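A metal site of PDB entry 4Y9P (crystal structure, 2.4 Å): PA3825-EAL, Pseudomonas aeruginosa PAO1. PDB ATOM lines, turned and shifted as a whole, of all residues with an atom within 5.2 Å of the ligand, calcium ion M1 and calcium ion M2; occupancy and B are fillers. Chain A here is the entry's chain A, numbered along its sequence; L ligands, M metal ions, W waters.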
ATOM      1  N   GLN A  25      -4.667  24.636  15.138  1.00  0.00           N
ATOM      2  CA  GLN A  25      -5.745  25.334  15.822  1.00  0.00           C
ATOM      3  C   GLN A  25      -6.746  24.333  16.480  1.00  0.00           C
ATOM      4  O   GLN A  25      -7.389  23.504  15.760  1.00  0.00           O
ATOM      5  CB  GLN A  25      -6.535  26.281  14.881  1.00  0.00           C
ATOM      6  CG  GLN A  25      -7.535  27.119  15.701  1.00  0.00           C
ATOM      7  CD  GLN A  25      -8.217  28.245  14.949  1.00  0.00           C
ATOM      8  OE1 GLN A  25      -8.559  28.073  13.815  1.00  0.00           O
ATOM      9  NE2 GLN A  25      -8.498  29.359  15.623  1.00  0.00           N
ATOM     10  N   GLU A  39      -7.096  21.688  13.533  1.00  0.00           N
ATOM     11  CA  GLU A  39      -6.902  21.990  12.096  1.00  0.00           C
ATOM     12  C   GLU A  39      -5.464  22.339  11.927  1.00  0.00           C
ATOM     13  O   GLU A  39      -4.944  23.148  12.687  1.00  0.00           O
ATOM     14  CB  GLU A  39      -7.784  23.170  11.595  1.00  0.00           C
ATOM     15  CG  GLU A  39      -7.739  23.336  10.073  1.00  0.00           C
ATOM     16  CD  GLU A  39      -8.516  24.539   9.505  1.00  0.00           C
ATOM     17  OE1 GLU A  39      -9.201  25.222  10.295  1.00  0.00           O
ATOM     18  OE2 GLU A  39      -8.413  24.779   8.240  1.00  0.00           O
ATOM     19  N   VAL A  40      -4.809  21.705  10.968  1.00  0.00           N
ATOM     20  CA  VAL A  40      -3.441  21.965  10.718  1.00  0.00           C
ATOM     21  C   VAL A  40      -3.396  23.101   9.748  1.00  0.00           C
ATOM     22  O   VAL A  40      -4.003  22.975   8.656  1.00  0.00           O
ATOM     23  CB  VAL A  40      -2.768  20.751  10.048  1.00  0.00           C
ATOM     24  CG1 VAL A  40      -1.370  21.116   9.592  1.00  0.00           C
ATOM     25  CG2 VAL A  40      -2.798  19.600  11.025  1.00  0.00           C
ATOM     26  N   LEU A  41      -2.734  24.188  10.124  1.00  0.00           N
ATOM     27  CA  LEU A  41      -2.591  25.374   9.243  1.00  0.00           C
ATOM     28  C   LEU A  41      -1.125  25.618   8.823  1.00  0.00           C
ATOM     29  O   LEU A  41      -0.230  25.601   9.650  1.00  0.00           O
ATOM     30  CB  LEU A  41      -3.119  26.619   9.965  1.00  0.00           C
ATOM     31  CG  LEU A  41      -4.595  26.949  10.155  1.00  0.00           C
ATOM     32  CD1 LEU A  41      -5.532  25.887   9.654  1.00  0.00           C
ATOM     33  CD2 LEU A  41      -4.840  27.236  11.620  1.00  0.00           C
ATOM     34  N   MET A  42      -0.889  25.819   7.545  1.00  0.00           N
ATOM     35  CA  MET A  42       0.457  25.989   7.091  1.00  0.00           C
ATOM     36  C   MET A  42       1.025  27.334   7.476  1.00  0.00           C
ATOM     37  O   MET A  42       0.359  28.348   7.459  1.00  0.00           O
ATOM     38  CB  MET A  42       0.556  25.819   5.590  1.00  0.00           C
ATOM     39  CG  MET A  42       1.973  25.505   5.139  1.00  0.00           C
ATOM     40  SD  MET A  42       2.063  25.106   3.349  1.00  0.00           S
ATOM     41  CE  MET A  42       0.945  23.720   3.168  1.00  0.00           C
ATOM     42  N   ARG A  43       2.288  27.324   7.823  1.00  0.00           N
ATOM     43  CA  ARG A  43       3.018  28.537   8.060  1.00  0.00           C
ATOM     44  C   ARG A  43       4.317  28.418   7.355  1.00  0.00           C
ATOM     45  O   ARG A  43       4.886  27.320   7.259  1.00  0.00           O
ATOM     46  CB  ARG A  43       3.229  28.741   9.575  1.00  0.00           C
ATOM     47  CG  ARG A  43       1.961  29.059  10.371  1.00  0.00           C
ATOM     48  CD  ARG A  43       1.467  30.472  10.110  1.00  0.00           C
ATOM     49  NE  ARG A  43       0.242  30.810  10.855  1.00  0.00           N
ATOM     50  CZ  ARG A  43      -1.009  30.489  10.482  1.00  0.00           C
ATOM     51  NH1 ARG A  43      -1.249  29.826   9.361  1.00  0.00           N
ATOM     52  NH2 ARG A  43      -2.041  30.881  11.219  1.00  0.00           N
ATOM     53  N   ARG A  53       2.269  34.200   6.401  1.00  0.00           N
ATOM     54  CA  ARG A  53       0.986  33.523   6.486  1.00  0.00           C
ATOM     55  C   ARG A  53       0.472  33.072   5.124  1.00  0.00           C
ATOM     56  O   ARG A  53       0.834  33.658   4.092  1.00  0.00           O
ATOM     57  CB  ARG A  53      -0.017  34.409   7.132  1.00  0.00           C
ATOM     58  CG  ARG A  53      -0.372  34.019   8.549  1.00  0.00           C
ATOM     59  CD  ARG A  53      -1.590  34.855   8.938  1.00  0.00           C
ATOM     60  NE  ARG A  53      -2.456  34.153   9.856  1.00  0.00           N
ATOM     61  CZ  ARG A  53      -3.759  34.351  10.015  1.00  0.00           C
ATOM     62  NH1 ARG A  53      -4.451  35.254   9.316  1.00  0.00           N
ATOM     63  NH2 ARG A  53      -4.407  33.595  10.917  1.00  0.00           N
ATOM     64  N   PRO A  54      -0.359  32.036   5.119  1.00  0.00           N
ATOM     65  CA  PRO A  54      -0.806  31.310   3.908  1.00  0.00           C
ATOM     66  C   PRO A  54      -1.297  32.114   2.724  1.00  0.00           C
ATOM     67  O   PRO A  54      -1.009  31.757   1.567  1.00  0.00           O
ATOM     68  CB  PRO A  54      -1.949  30.416   4.407  1.00  0.00           C
ATOM     69  CG  PRO A  54      -1.707  30.241   5.878  1.00  0.00           C
ATOM     70  CD  PRO A  54      -0.972  31.454   6.352  1.00  0.00           C
ATOM     71  N   ASP A  55      -2.071  33.157   2.995  1.00  0.00           N
ATOM     72  CA  ASP A  55      -2.705  33.920   1.921  1.00  0.00           C
ATOM     73  C   ASP A  55      -1.700  34.635   1.070  1.00  0.00           C
ATOM     74  O   ASP A  55      -1.992  34.911  -0.061  1.00  0.00           O
ATOM     75  CB  ASP A  55      -3.792  34.887   2.459  1.00  0.00           C
ATOM     76  CG  ASP A  55      -5.036  34.131   3.038  1.00  0.00           C
ATOM     77  OD1 ASP A  55      -5.259  32.922   2.750  1.00  0.00           O
ATOM     78  OD2 ASP A  55      -5.798  34.757   3.795  1.00  0.00           O
ATOM     79  N   ILE A  58      -0.077  30.425  -0.530  1.00  0.00           N
ATOM     80  CA  ILE A  58      -0.901  29.313  -1.038  1.00  0.00           C
ATOM     81  C   ILE A  58      -1.440  29.551  -2.447  1.00  0.00           C
ATOM     82  O   ILE A  58      -1.427  28.637  -3.265  1.00  0.00           O
ATOM     83  CB  ILE A  58      -2.056  28.947  -0.079  1.00  0.00           C
ATOM     84  CG1 ILE A  58      -1.522  28.300   1.190  1.00  0.00           C
ATOM     85  CG2 ILE A  58      -3.058  28.013  -0.747  1.00  0.00           C
ATOM     86  CD1 ILE A  58      -0.933  26.919   1.010  1.00  0.00           C
ATOM     87  N   GLU A  62      -0.715  26.793  -5.506  1.00  0.00           N
ATOM     88  CA  GLU A  62      -1.807  26.137  -6.234  1.00  0.00           C
ATOM     89  C   GLU A  62      -1.644  26.268  -7.725  1.00  0.00           C
ATOM     90  O   GLU A  62      -1.757  25.284  -8.418  1.00  0.00           O
ATOM     91  CB  GLU A  62      -3.187  26.632  -5.749  1.00  0.00           C
ATOM     92  CG  GLU A  62      -3.470  26.162  -4.317  1.00  0.00           C
ATOM     93  CD  GLU A  62      -4.811  26.590  -3.743  1.00  0.00           C
ATOM     94  OE1 GLU A  62      -5.357  27.647  -4.134  1.00  0.00           O
ATOM     95  OE2 GLU A  62      -5.314  25.870  -2.827  1.00  0.00           O
ATOM     96  N   ILE A  67       1.680  23.002  -4.325  1.00  0.00           N
ATOM     97  CA  ILE A  67       0.846  22.788  -3.131  1.00  0.00           C
ATOM     98  C   ILE A  67       0.666  21.310  -2.780  1.00  0.00           C
ATOM     99  O   ILE A  67       0.600  20.928  -1.596  1.00  0.00           O
ATOM    100  CB  ILE A  67      -0.526  23.494  -3.265  1.00  0.00           C
ATOM    101  CG1 ILE A  67      -1.303  23.457  -1.938  1.00  0.00           C
ATOM    102  CG2 ILE A  67      -1.364  22.886  -4.375  1.00  0.00           C
ATOM    103  CD1 ILE A  67      -0.578  24.103  -0.771  1.00  0.00           C
ATOM    104  N   THR A  71       1.783  19.903   0.818  1.00  0.00           N
ATOM    105  CA  THR A  71       0.822  19.308   1.713  1.00  0.00           C
ATOM    106  C   THR A  71       1.314  17.940   2.209  1.00  0.00           C
ATOM    107  O   THR A  71       1.095  17.533   3.378  1.00  0.00           O
ATOM    108  CB  THR A  71      -0.501  19.205   0.957  1.00  0.00           C
ATOM    109  OG1 THR A  71      -0.876  20.516   0.537  1.00  0.00           O
ATOM    110  CG2 THR A  71      -1.578  18.570   1.793  1.00  0.00           C
ATOM    111  N   LEU A  74       3.764  18.439   4.929  1.00  0.00           N
ATOM    112  CA  LEU A  74       3.049  18.896   6.136  1.00  0.00           C
ATOM    113  C   LEU A  74       2.442  17.705   6.872  1.00  0.00           C
ATOM    114  O   LEU A  74       2.623  17.567   8.060  1.00  0.00           O
ATOM    115  CB  LEU A  74       1.959  19.899   5.744  1.00  0.00           C
ATOM    116  CG  LEU A  74       1.510  20.831   6.858  1.00  0.00           C
ATOM    117  CD1 LEU A  74       2.575  21.904   7.102  1.00  0.00           C
ATOM    118  CD2 LEU A  74       0.176  21.461   6.454  1.00  0.00           C
ATOM    119  N   ASN A  98      -6.144  21.169   5.126  1.00  0.00           N
ATOM    120  CA  ASN A  98      -6.762  21.857   4.022  1.00  0.00           C
ATOM    121  C   ASN A  98      -6.197  21.263   2.731  1.00  0.00           C
ATOM    122  O   ASN A  98      -5.014  21.106   2.623  1.00  0.00           O
ATOM    123  CB  ASN A  98      -6.454  23.360   4.116  1.00  0.00           C
ATOM    124  CG  ASN A  98      -7.111  23.973   5.311  1.00  0.00           C
ATOM    125  OD1 ASN A  98      -8.311  24.214   5.287  1.00  0.00           O
ATOM    126  ND2 ASN A  98      -6.349  24.196   6.381  1.00  0.00           N
ATOM    127  N   ILE A  99      -7.046  20.957   1.759  1.00  0.00           N
ATOM    128  CA  ILE A  99      -6.691  20.228   0.509  1.00  0.00           C
ATOM    129  C   ILE A  99      -7.072  21.105  -0.662  1.00  0.00           C
ATOM    130  O   ILE A  99      -8.126  21.706  -0.651  1.00  0.00           O
ATOM    131  CB  ILE A  99      -7.551  18.917   0.480  1.00  0.00           C
ATOM    132  CG1 ILE A  99      -7.034  17.848   1.470  1.00  0.00           C
ATOM    133  CG2 ILE A  99      -7.666  18.250  -0.867  1.00  0.00           C
ATOM    134  CD1 ILE A  99      -5.547  17.756   1.644  1.00  0.00           C
ATOM    135  N   SER A 100      -6.231  21.174  -1.690  1.00  0.00           N
ATOM    136  CA  SER A 100      -6.548  21.921  -2.900  1.00  0.00           C
ATOM    137  C   SER A 100      -7.321  21.095  -3.934  1.00  0.00           C
ATOM    138  O   SER A 100      -7.380  19.883  -3.866  1.00  0.00           O
ATOM    139  CB  SER A 100      -5.297  22.526  -3.561  1.00  0.00           C
ATOM    140  OG  SER A 100      -4.197  21.704  -3.320  1.00  0.00           O
ATOM    141  N   GLU A 130     -10.369  19.023   4.272  1.00  0.00           N
ATOM    142  CA  GLU A 130     -11.225  20.176   4.110  1.00  0.00           C
ATOM    143  C   GLU A 130     -11.051  20.683   2.710  1.00  0.00           C
ATOM    144  O   GLU A 130      -9.940  20.961   2.252  1.00  0.00           O
ATOM    145  CB  GLU A 130     -10.918  21.271   5.146  1.00  0.00           C
ATOM    146  CG  GLU A 130     -10.698  20.782   6.556  1.00  0.00           C
ATOM    147  CD  GLU A 130     -10.614  21.912   7.582  1.00  0.00           C
ATOM    148  OE1 GLU A 130     -10.544  23.108   7.190  1.00  0.00           O
ATOM    149  OE2 GLU A 130     -10.659  21.595   8.811  1.00  0.00           O
ATOM    150  N   ASP A 160     -15.153  23.302   3.670  1.00  0.00           N
ATOM    151  CA  ASP A 160     -14.584  24.460   4.337  1.00  0.00           C
ATOM    152  C   ASP A 160     -15.356  25.654   3.906  1.00  0.00           C
ATOM    153  O   ASP A 160     -15.923  25.642   2.824  1.00  0.00           O
ATOM    154  CB  ASP A 160     -13.149  24.653   3.912  1.00  0.00           C
ATOM    155  CG  ASP A 160     -12.296  25.249   4.975  1.00  0.00           C
ATOM    156  OD1 ASP A 160     -12.794  25.944   5.872  1.00  0.00           O
ATOM    157  OD2 ASP A 160     -11.096  24.983   4.908  1.00  0.00           O
ATOM    158  N   ASP A 161     -15.385  26.668   4.750  1.00  0.00           N
ATOM    159  CA  ASP A 161     -15.976  27.989   4.372  1.00  0.00           C
ATOM    160  C   ASP A 161     -17.349  27.865   3.716  1.00  0.00           C
ATOM    161  O   ASP A 161     -17.615  28.469   2.682  1.00  0.00           O
ATOM    162  CB  ASP A 161     -14.990  28.779   3.481  1.00  0.00           C
ATOM    163  CG  ASP A 161     -13.611  28.999   4.167  1.00  0.00           C
ATOM    164  OD1 ASP A 161     -13.455  29.069   5.458  1.00  0.00           O
ATOM    165  OD2 ASP A 161     -12.677  29.099   3.339  1.00  0.00           O
ATOM    166  N   LYS A 181     -18.070  22.963   7.626  1.00  0.00           N
ATOM    167  CA  LYS A 181     -17.518  24.073   8.423  1.00  0.00           C
ATOM    168  C   LYS A 181     -18.109  25.418   8.040  1.00  0.00           C
ATOM    169  O   LYS A 181     -17.951  25.935   6.932  1.00  0.00           O
ATOM    170  CB  LYS A 181     -16.025  24.111   8.272  1.00  0.00           C
ATOM    171  CG  LYS A 181     -15.432  22.760   8.572  1.00  0.00           C
ATOM    172  CD  LYS A 181     -13.924  22.812   8.671  1.00  0.00           C
ATOM    173  CE  LYS A 181     -13.433  23.374   9.964  1.00  0.00           C
ATOM    174  NZ  LYS A 181     -12.020  23.763   9.857  1.00  0.00           N
ATOM    175  N   ASP A 183     -18.308  29.013   7.560  1.00  0.00           N
ATOM    176  CA  ASP A 183     -17.376  30.156   7.461  1.00  0.00           C
ATOM    177  C   ASP A 183     -17.514  31.199   8.594  1.00  0.00           C
ATOM    178  O   ASP A 183     -18.639  31.559   9.036  1.00  0.00           O
ATOM    179  CB  ASP A 183     -17.600  30.884   6.157  1.00  0.00           C
ATOM    180  CG  ASP A 183     -16.474  31.850   5.836  1.00  0.00           C
ATOM    181  OD1 ASP A 183     -15.333  31.371   5.620  1.00  0.00           O
ATOM    182  OD2 ASP A 183     -16.776  33.057   5.791  1.00  0.00           O
ATOM    183  N   GLN A 184     -16.396  31.764   8.967  1.00  0.00           N
ATOM    184  CA  GLN A 184     -16.365  32.836   9.981  1.00  0.00           C
ATOM    185  C   GLN A 184     -17.188  34.061   9.683  1.00  0.00           C
ATOM    186  O   GLN A 184     -17.604  34.773  10.600  1.00  0.00           O
ATOM    187  CB  GLN A 184     -14.913  33.218  10.356  1.00  0.00           C
ATOM    188  CG  GLN A 184     -13.834  33.133   9.262  1.00  0.00           C
ATOM    189  CD  GLN A 184     -12.397  33.084   9.779  1.00  0.00           C
ATOM    190  OE1 GLN A 184     -11.732  34.117   9.821  1.00  0.00           O
ATOM    191  NE2 GLN A 184     -11.893  31.879  10.186  1.00  0.00           N
ATOM    192  N   GLU A 217     -16.544  28.047  12.657  1.00  0.00           N
ATOM    193  CA  GLU A 217     -15.213  28.705  12.603  1.00  0.00           C
ATOM    194  C   GLU A 217     -15.309  30.163  12.982  1.00  0.00           C
ATOM    195  O   GLU A 217     -16.296  30.781  12.755  1.00  0.00           O
ATOM    196  CB  GLU A 217     -14.672  28.718  11.179  1.00  0.00           C
ATOM    197  CG  GLU A 217     -14.393  27.375  10.522  1.00  0.00           C
ATOM    198  CD  GLU A 217     -13.873  27.636   9.069  1.00  0.00           C
ATOM    199  OE1 GLU A 217     -12.849  28.347   8.861  1.00  0.00           O
ATOM    200  OE2 GLU A 217     -14.534  27.224   8.077  1.00  0.00           O
ATOM    201  N   GLY A 218     -14.276  30.693  13.610  1.00  0.00           N
ATOM    202  CA  GLY A 218     -14.202  32.085  13.982  1.00  0.00           C
ATOM    203  C   GLY A 218     -15.042  32.459  15.174  1.00  0.00           C
ATOM    204  O   GLY A 218     -15.471  33.609  15.300  1.00  0.00           O
ATOM    205  N   VAL A 219     -15.231  31.539  16.109  1.00  0.00           N
ATOM    206  CA  VAL A 219     -15.919  31.893  17.366  1.00  0.00           C
ATOM    207  C   VAL A 219     -14.948  32.714  18.236  1.00  0.00           C
ATOM    208  O   VAL A 219     -13.902  32.233  18.608  1.00  0.00           O
ATOM    209  CB  VAL A 219     -16.316  30.630  18.126  1.00  0.00           C
ATOM    210  CG1 VAL A 219     -17.058  30.955  19.407  1.00  0.00           C
ATOM    211  CG2 VAL A 219     -17.146  29.768  17.248  1.00  0.00           C
ATOM    212  N   GLU A 220     -15.263  33.946  18.449  1.00  0.00           N
ATOM    213  CA  GLU A 220     -14.457  34.868  19.248  1.00  0.00           C
ATOM    214  C   GLU A 220     -15.140  35.343  20.530  1.00  0.00           C
ATOM    215  O   GLU A 220     -14.473  35.761  21.462  1.00  0.00           O
ATOM    216  CB  GLU A 220     -14.137  36.136  18.398  1.00  0.00           C
ATOM    217  CG  GLU A 220     -13.422  35.788  17.125  1.00  0.00           C
ATOM    218  CD  GLU A 220     -13.191  36.972  16.208  1.00  0.00           C
ATOM    219  OE1 GLU A 220     -13.811  38.061  16.354  1.00  0.00           O
ATOM    220  OE2 GLU A 220     -12.401  36.789  15.256  1.00  0.00           O
ATOM    221  N   GLN A 237     -14.474  26.495  16.753  1.00  0.00           N
ATOM    222  CA  GLN A 237     -13.103  26.797  16.413  1.00  0.00           C
ATOM    223  C   GLN A 237     -13.026  28.306  16.343  1.00  0.00           C
ATOM    224  O   GLN A 237     -13.954  28.993  15.865  1.00  0.00           O
ATOM    225  CB  GLN A 237     -12.792  26.078  15.103  1.00  0.00           C
ATOM    226  CG  GLN A 237     -11.476  26.359  14.532  1.00  0.00           C
ATOM    227  CD  GLN A 237     -11.200  25.580  13.238  1.00  0.00           C
ATOM    228  OE1 GLN A 237     -12.010  24.757  12.748  1.00  0.00           O
ATOM    229  NE2 GLN A 237      -9.994  25.800  12.700  1.00  0.00           N
ATOM    230  N   GLY A 238     -11.949  28.845  16.874  1.00  0.00           N
ATOM    231  CA  GLY A 238     -11.803  30.308  16.844  1.00  0.00           C
ATOM    232  C   GLY A 238     -10.900  30.768  17.977  1.00  0.00           C
ATOM    233  O   GLY A 238     -10.528  29.954  18.825  1.00  0.00           O
ATOM    234  N   TYR A 239     -10.616  32.096  18.022  1.00  0.00           N
ATOM    235  CA  TYR A 239      -9.823  32.705  19.067  1.00  0.00           C
ATOM    236  C   TYR A 239     -10.404  32.490  20.432  1.00  0.00           C
ATOM    237  O   TYR A 239      -9.634  32.457  21.340  1.00  0.00           O
ATOM    238  CB  TYR A 239      -9.564  34.206  18.819  1.00  0.00           C
ATOM    239  CG  TYR A 239      -8.744  34.459  17.519  1.00  0.00           C
ATOM    240  CD1 TYR A 239      -7.924  33.466  16.966  1.00  0.00           C
ATOM    241  CD2 TYR A 239      -8.847  35.625  16.819  1.00  0.00           C
ATOM    242  CE1 TYR A 239      -7.195  33.682  15.834  1.00  0.00           C
ATOM    243  CE2 TYR A 239      -8.107  35.837  15.669  1.00  0.00           C
ATOM    244  CZ  TYR A 239      -7.261  34.850  15.193  1.00  0.00           C
ATOM    245  OH  TYR A 239      -6.495  34.944  14.030  1.00  0.00           O
ATOM    246  N   LEU A 240     -11.725  32.296  20.557  1.00  0.00           N
ATOM    247  CA  LEU A 240     -12.318  31.995  21.850  1.00  0.00           C
ATOM    248  C   LEU A 240     -11.764  30.695  22.425  1.00  0.00           C
ATOM    249  O   LEU A 240     -11.488  30.634  23.575  1.00  0.00           O
ATOM    250  CB  LEU A 240     -13.848  31.934  21.797  1.00  0.00           C
ATOM    251  CG  LEU A 240     -14.526  31.922  23.217  1.00  0.00           C
ATOM    252  CD1 LEU A 240     -15.074  33.252  23.643  1.00  0.00           C
ATOM    253  CD2 LEU A 240     -15.690  30.987  23.313  1.00  0.00           C
ATOM    254  N   PRO A 244      -4.274  29.503  16.332  1.00  0.00           N
ATOM    255  CA  PRO A 244      -3.342  28.584  15.696  1.00  0.00           C
ATOM    256  C   PRO A 244      -2.043  28.664  16.436  1.00  0.00           C
ATOM    257  O   PRO A 244      -1.686  29.738  16.823  1.00  0.00           O
ATOM    258  CB  PRO A 244      -3.166  29.152  14.310  1.00  0.00           C
ATOM    259  CG  PRO A 244      -4.375  29.957  14.052  1.00  0.00           C
ATOM    260  CD  PRO A 244      -4.851  30.459  15.382  1.00  0.00           C
HETATM  261  P1  LIG L   1      -9.409  28.543   6.448  1.00  0.00           P
HETATM  262  O1  LIG L   1      -8.855  27.159   6.375  1.00  0.00           O
HETATM  263  O2  LIG L   1     -10.841  28.757   6.000  1.00  0.00           O
HETATM  264  O3  LIG L   1      -9.534  29.217   7.869  1.00  0.00           O
HETATM  265  C1  LIG L   1      -8.539  29.238   8.835  1.00  0.00           C
HETATM  266  C2  LIG L   1      -8.139  30.697   8.934  1.00  0.00           C
HETATM  267  O4  LIG L   1      -8.865  31.501   9.874  1.00  0.00           O
HETATM  268  C3  LIG L   1      -6.732  30.703   9.435  1.00  0.00           C
HETATM  269  O5  LIG L   1      -6.000  31.738   8.797  1.00  0.00           O
HETATM  270  C4  LIG L   1      -6.902  30.958  10.883  1.00  0.00           C
HETATM  271  O6  LIG L   1      -5.691  31.419  11.414  1.00  0.00           O
HETATM  272  C5  LIG L   1      -7.980  32.003  10.872  1.00  0.00           C
HETATM  273  N1  LIG L   1      -8.738  32.102  12.119  1.00  0.00           N
HETATM  274  C6  LIG L   1      -8.932  31.143  13.020  1.00  0.00           C
HETATM  275  N2  LIG L   1      -9.741  31.526  14.023  1.00  0.00           N
HETATM  276  C7  LIG L   1     -10.064  32.761  13.781  1.00  0.00           C
HETATM  277  C8  LIG L   1     -10.886  33.732  14.474  1.00  0.00           C
HETATM  278  O7  LIG L   1     -11.447  33.421  15.546  1.00  0.00           O
HETATM  279  N3  LIG L   1     -11.000  34.919  13.897  1.00  0.00           N
HETATM  280  C9  LIG L   1     -10.390  35.242  12.722  1.00  0.00           C
HETATM  281  N4  LIG L   1     -10.563  36.484  12.226  1.00  0.00           N
HETATM  282  N5  LIG L   1      -9.610  34.377  12.021  1.00  0.00           N
HETATM  283  C10 LIG L   1      -9.408  33.152  12.522  1.00  0.00           C
HETATM  284  P2  LIG L   1      -4.590  31.328   8.151  1.00  0.00           P
HETATM  285  O8  LIG L   1      -3.839  30.327   9.024  1.00  0.00           O
HETATM  286  O9  LIG L   1      -3.960  32.584   7.626  1.00  0.00           O
HETATM  287  O10 LIG L   1      -5.132  30.492   6.885  1.00  0.00           O
HETATM  288  C11 LIG L   1      -5.983  31.198   5.947  1.00  0.00           C
HETATM  289  C12 LIG L   1      -6.377  30.273   4.823  1.00  0.00           C
HETATM  290  O11 LIG L   1      -5.223  29.725   4.208  1.00  0.00           O
HETATM  291  C13 LIG L   1      -7.124  29.078   5.331  1.00  0.00           C
HETATM  292  O12 LIG L   1      -8.443  29.490   5.602  1.00  0.00           O
HETATM  293  C14 LIG L   1      -6.891  28.116   4.200  1.00  0.00           C
HETATM  294  O13 LIG L   1      -7.699  28.430   3.100  1.00  0.00           O
HETATM  295  C15 LIG L   1      -5.491  28.405   3.716  1.00  0.00           C
HETATM  296  N6  LIG L   1      -4.541  27.368   4.182  1.00  0.00           N
HETATM  297  C16 LIG L   1      -3.830  27.306   5.328  1.00  0.00           C
HETATM  298  N7  LIG L   1      -3.043  26.199   5.356  1.00  0.00           N
HETATM  299  C17 LIG L   1      -3.280  25.552   4.201  1.00  0.00           C
HETATM  300  C18 LIG L   1      -2.804  24.341   3.558  1.00  0.00           C
HETATM  301  O14 LIG L   1      -1.986  23.647   4.214  1.00  0.00           O
HETATM  302  N8  LIG L   1      -3.270  24.029   2.319  1.00  0.00           N
HETATM  303  C19 LIG L   1      -4.166  24.785   1.663  1.00  0.00           C
HETATM  304  N9  LIG L   1      -4.644  24.442   0.443  1.00  0.00           N
HETATM  305  N10 LIG L   1      -4.635  25.916   2.213  1.00  0.00           N
HETATM  306  C20 LIG L   1      -4.248  26.320   3.436  1.00  0.00           C
HETATM  307 CA    CA M   1      -9.881  25.266   6.696  1.00  0.00          CA
HETATM  308 CA    CA M   2     -13.109  30.134   7.335  1.00  0.00          CA
HETATM  309 CA    CA M   3      -8.347  24.683   0.597  1.00  0.00          CA
HETATM  310  O   HOH W   1      -3.798  21.971   6.174  1.00  0.00           O
HETATM  311  O   HOH W   2     -11.106  25.990   8.510  1.00  0.00           O
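The backbone carbonyl oxygen (O) of Gln 237 is in hydrogen-bond range of the backbone NH (N) of Gly 218 (2.8 Å).
The backbone NH (N) of Ile 99 is in hydrogen-bond range of the backbone carbonyl oxygen (O) of Glu 130, at 2.9 Å.
The side-chain carboxylate (OE1) of Glu 39 is in hydrogen-bond range of the side-chain amide nitrogen (NE2) of Gln 237 (2.6 Å).
The backbone NH (N) of Gln 25 lies within hydrogen-bond range of the backbone carbonyl oxygen (O) of Glu 39 (2.9 Å).
The backbone NH (N) of Asp 161 lies within hydrogen-bond range of the backbone carbonyl oxygen (O) of Lys 181, 3.4 Å away.
The backbone carbonyl oxygen of Val 40 lies within hydrogen-bond range of the side-chain amide nitrogen of Asn 98.
The side-chain amide nitrogen (NE2) of Gln 237 lies within hydrogen-bond range of the side-chain amide oxygen (OE1) of Gln 25 (2.9 Å).
N of Tyr 239 lies within hydrogen-bond range of O of Val 219, at 3.3 Å.
Merely in contact with calcium ion M2: Gln 184 (3.6 Å).
The nearest printed residue that does not touch calcium ion M2 is Asp 160 (4.4 Å).
Leu 41 touches the ligand.
Pro 54 touches the ligand (CB to O11, 3.4 Å).
OD1 of Asp 55 touches O11 of the ligand (3.5 Å).
Ile 58 touches the ligand (CD1 to C19, 3.9 Å).
OE2 of Glu 62 touches N9 of the ligand, 3.6 Å away.
Leu 74 touches the ligand (CD2 to O14, 3.8 Å).
Gly 218 touches the ligand (CA to O7, 3.4 Å).
CA of Gly 238 touches O7 of the ligand, at 3.4 Å.
Pro 244 touches the ligand (CG to O6, 3.3 Å).
Hydrophobic or aromatic side chains within 4 Å of the ligand: Leu 41, Met 42, Pro 54, Ile 58, Leu 74, Tyr 239 and Pro 244.
21 residues have an atom within 4 Å of the ligand: Gln 25, Glu 39, Leu 41, Met 42, Arg 43, Arg 53, Pro 54, Asp 55, Ile 58, Glu 62, Leu 74, Asn 98, Asp 160, Asp 161, Gln 184, Glu 217, Gly 218, Glu 220, Gly 238, Tyr 239 and Pro 244.
Four residues have an atom within 4 Å of calcium ion M1: Glu 39, Asn 98, Glu 130 and Asp 160.
The nearest printed residue that does not touch calcium ion M1 is Lys 181 (4.1 Å).
NE2 of Gln 25 lies within hydrogen-bond range of N2 of the ligand.
The backbone carbonyl oxygen (O) of Asn 98 sits at hydrogen-bond distance from a nitrogen (N8) of the ligand.
The side-chain carboxylate (OD1) of Asp 161 lies close to an oxygen (O2) of the ligand (2.7 Å).
An oxygen (O4) of the ligand lies within hydrogen-bond range of the side-chain amide nitrogen of Gln 184 (3.1 Å).
A nitrogen (N3) of the ligand is in hydrogen-bond range of the side-chain carboxylate (OE2) of Glu 220 (2.7 Å).
An oxygen (O9) of the ligand is in salt-bridge range of the guanidinium group (NE) of Arg 53 (3.1 Å).
An oxygen (O7) of the ligand sits at hydrogen-bond distance from the backbone NH of Tyr 239, at 2.9 Å.
N of Met 42 sits at hydrogen-bond distance from N7 of the ligand (3.1 Å).
NH1 of Arg 43 is in salt-bridge range of O8 of the ligand (2.7 Å).
The side-chain carboxylate (OD1) of Asp 161 binds calcium ion M2.
Calcium ion M2 is bound by OE1 of Glu 217.
Slightly farther from calcium ion M2 lies O2 of the ligand (3.0 Å).
Slightly farther from calcium ion M2 lies OD1 of Asp 183 (3.1 Å).
Water W2 lies within hydrogen-bond range of OE1 of Glu 39 (2.7 Å), NZ of Lys 181 (2.8 Å) and OD1 of Asp 160 (3.1 Å).
Water W1 lies within hydrogen-bond range of the backbone carbonyl oxygen of Val 40 (2.7 Å), the backbone NH of Asn 98 (2.7 Å) and an oxygen (O14) of the ligand (3.2 Å).
Calcium ion M1 is bound by an oxygen (O1) of the ligand (2.2 Å), the side-chain carboxylate (OD2) of Asp 160 (2.2 Å), the side-chain carboxylate (OE2) of Glu 39 (2.2 Å), water W2 (2.3 Å), the side-chain carboxylate (OE1) of Glu 130 (2.3 Å) and the side-chain amide oxygen (OD1) of Asn 98 (2.4 Å).
Calcium ion M1 has six donor atoms within binding distance.
Slightly farther from calcium ion M1 lies OD1 of Asp 160 (3.1 Å).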
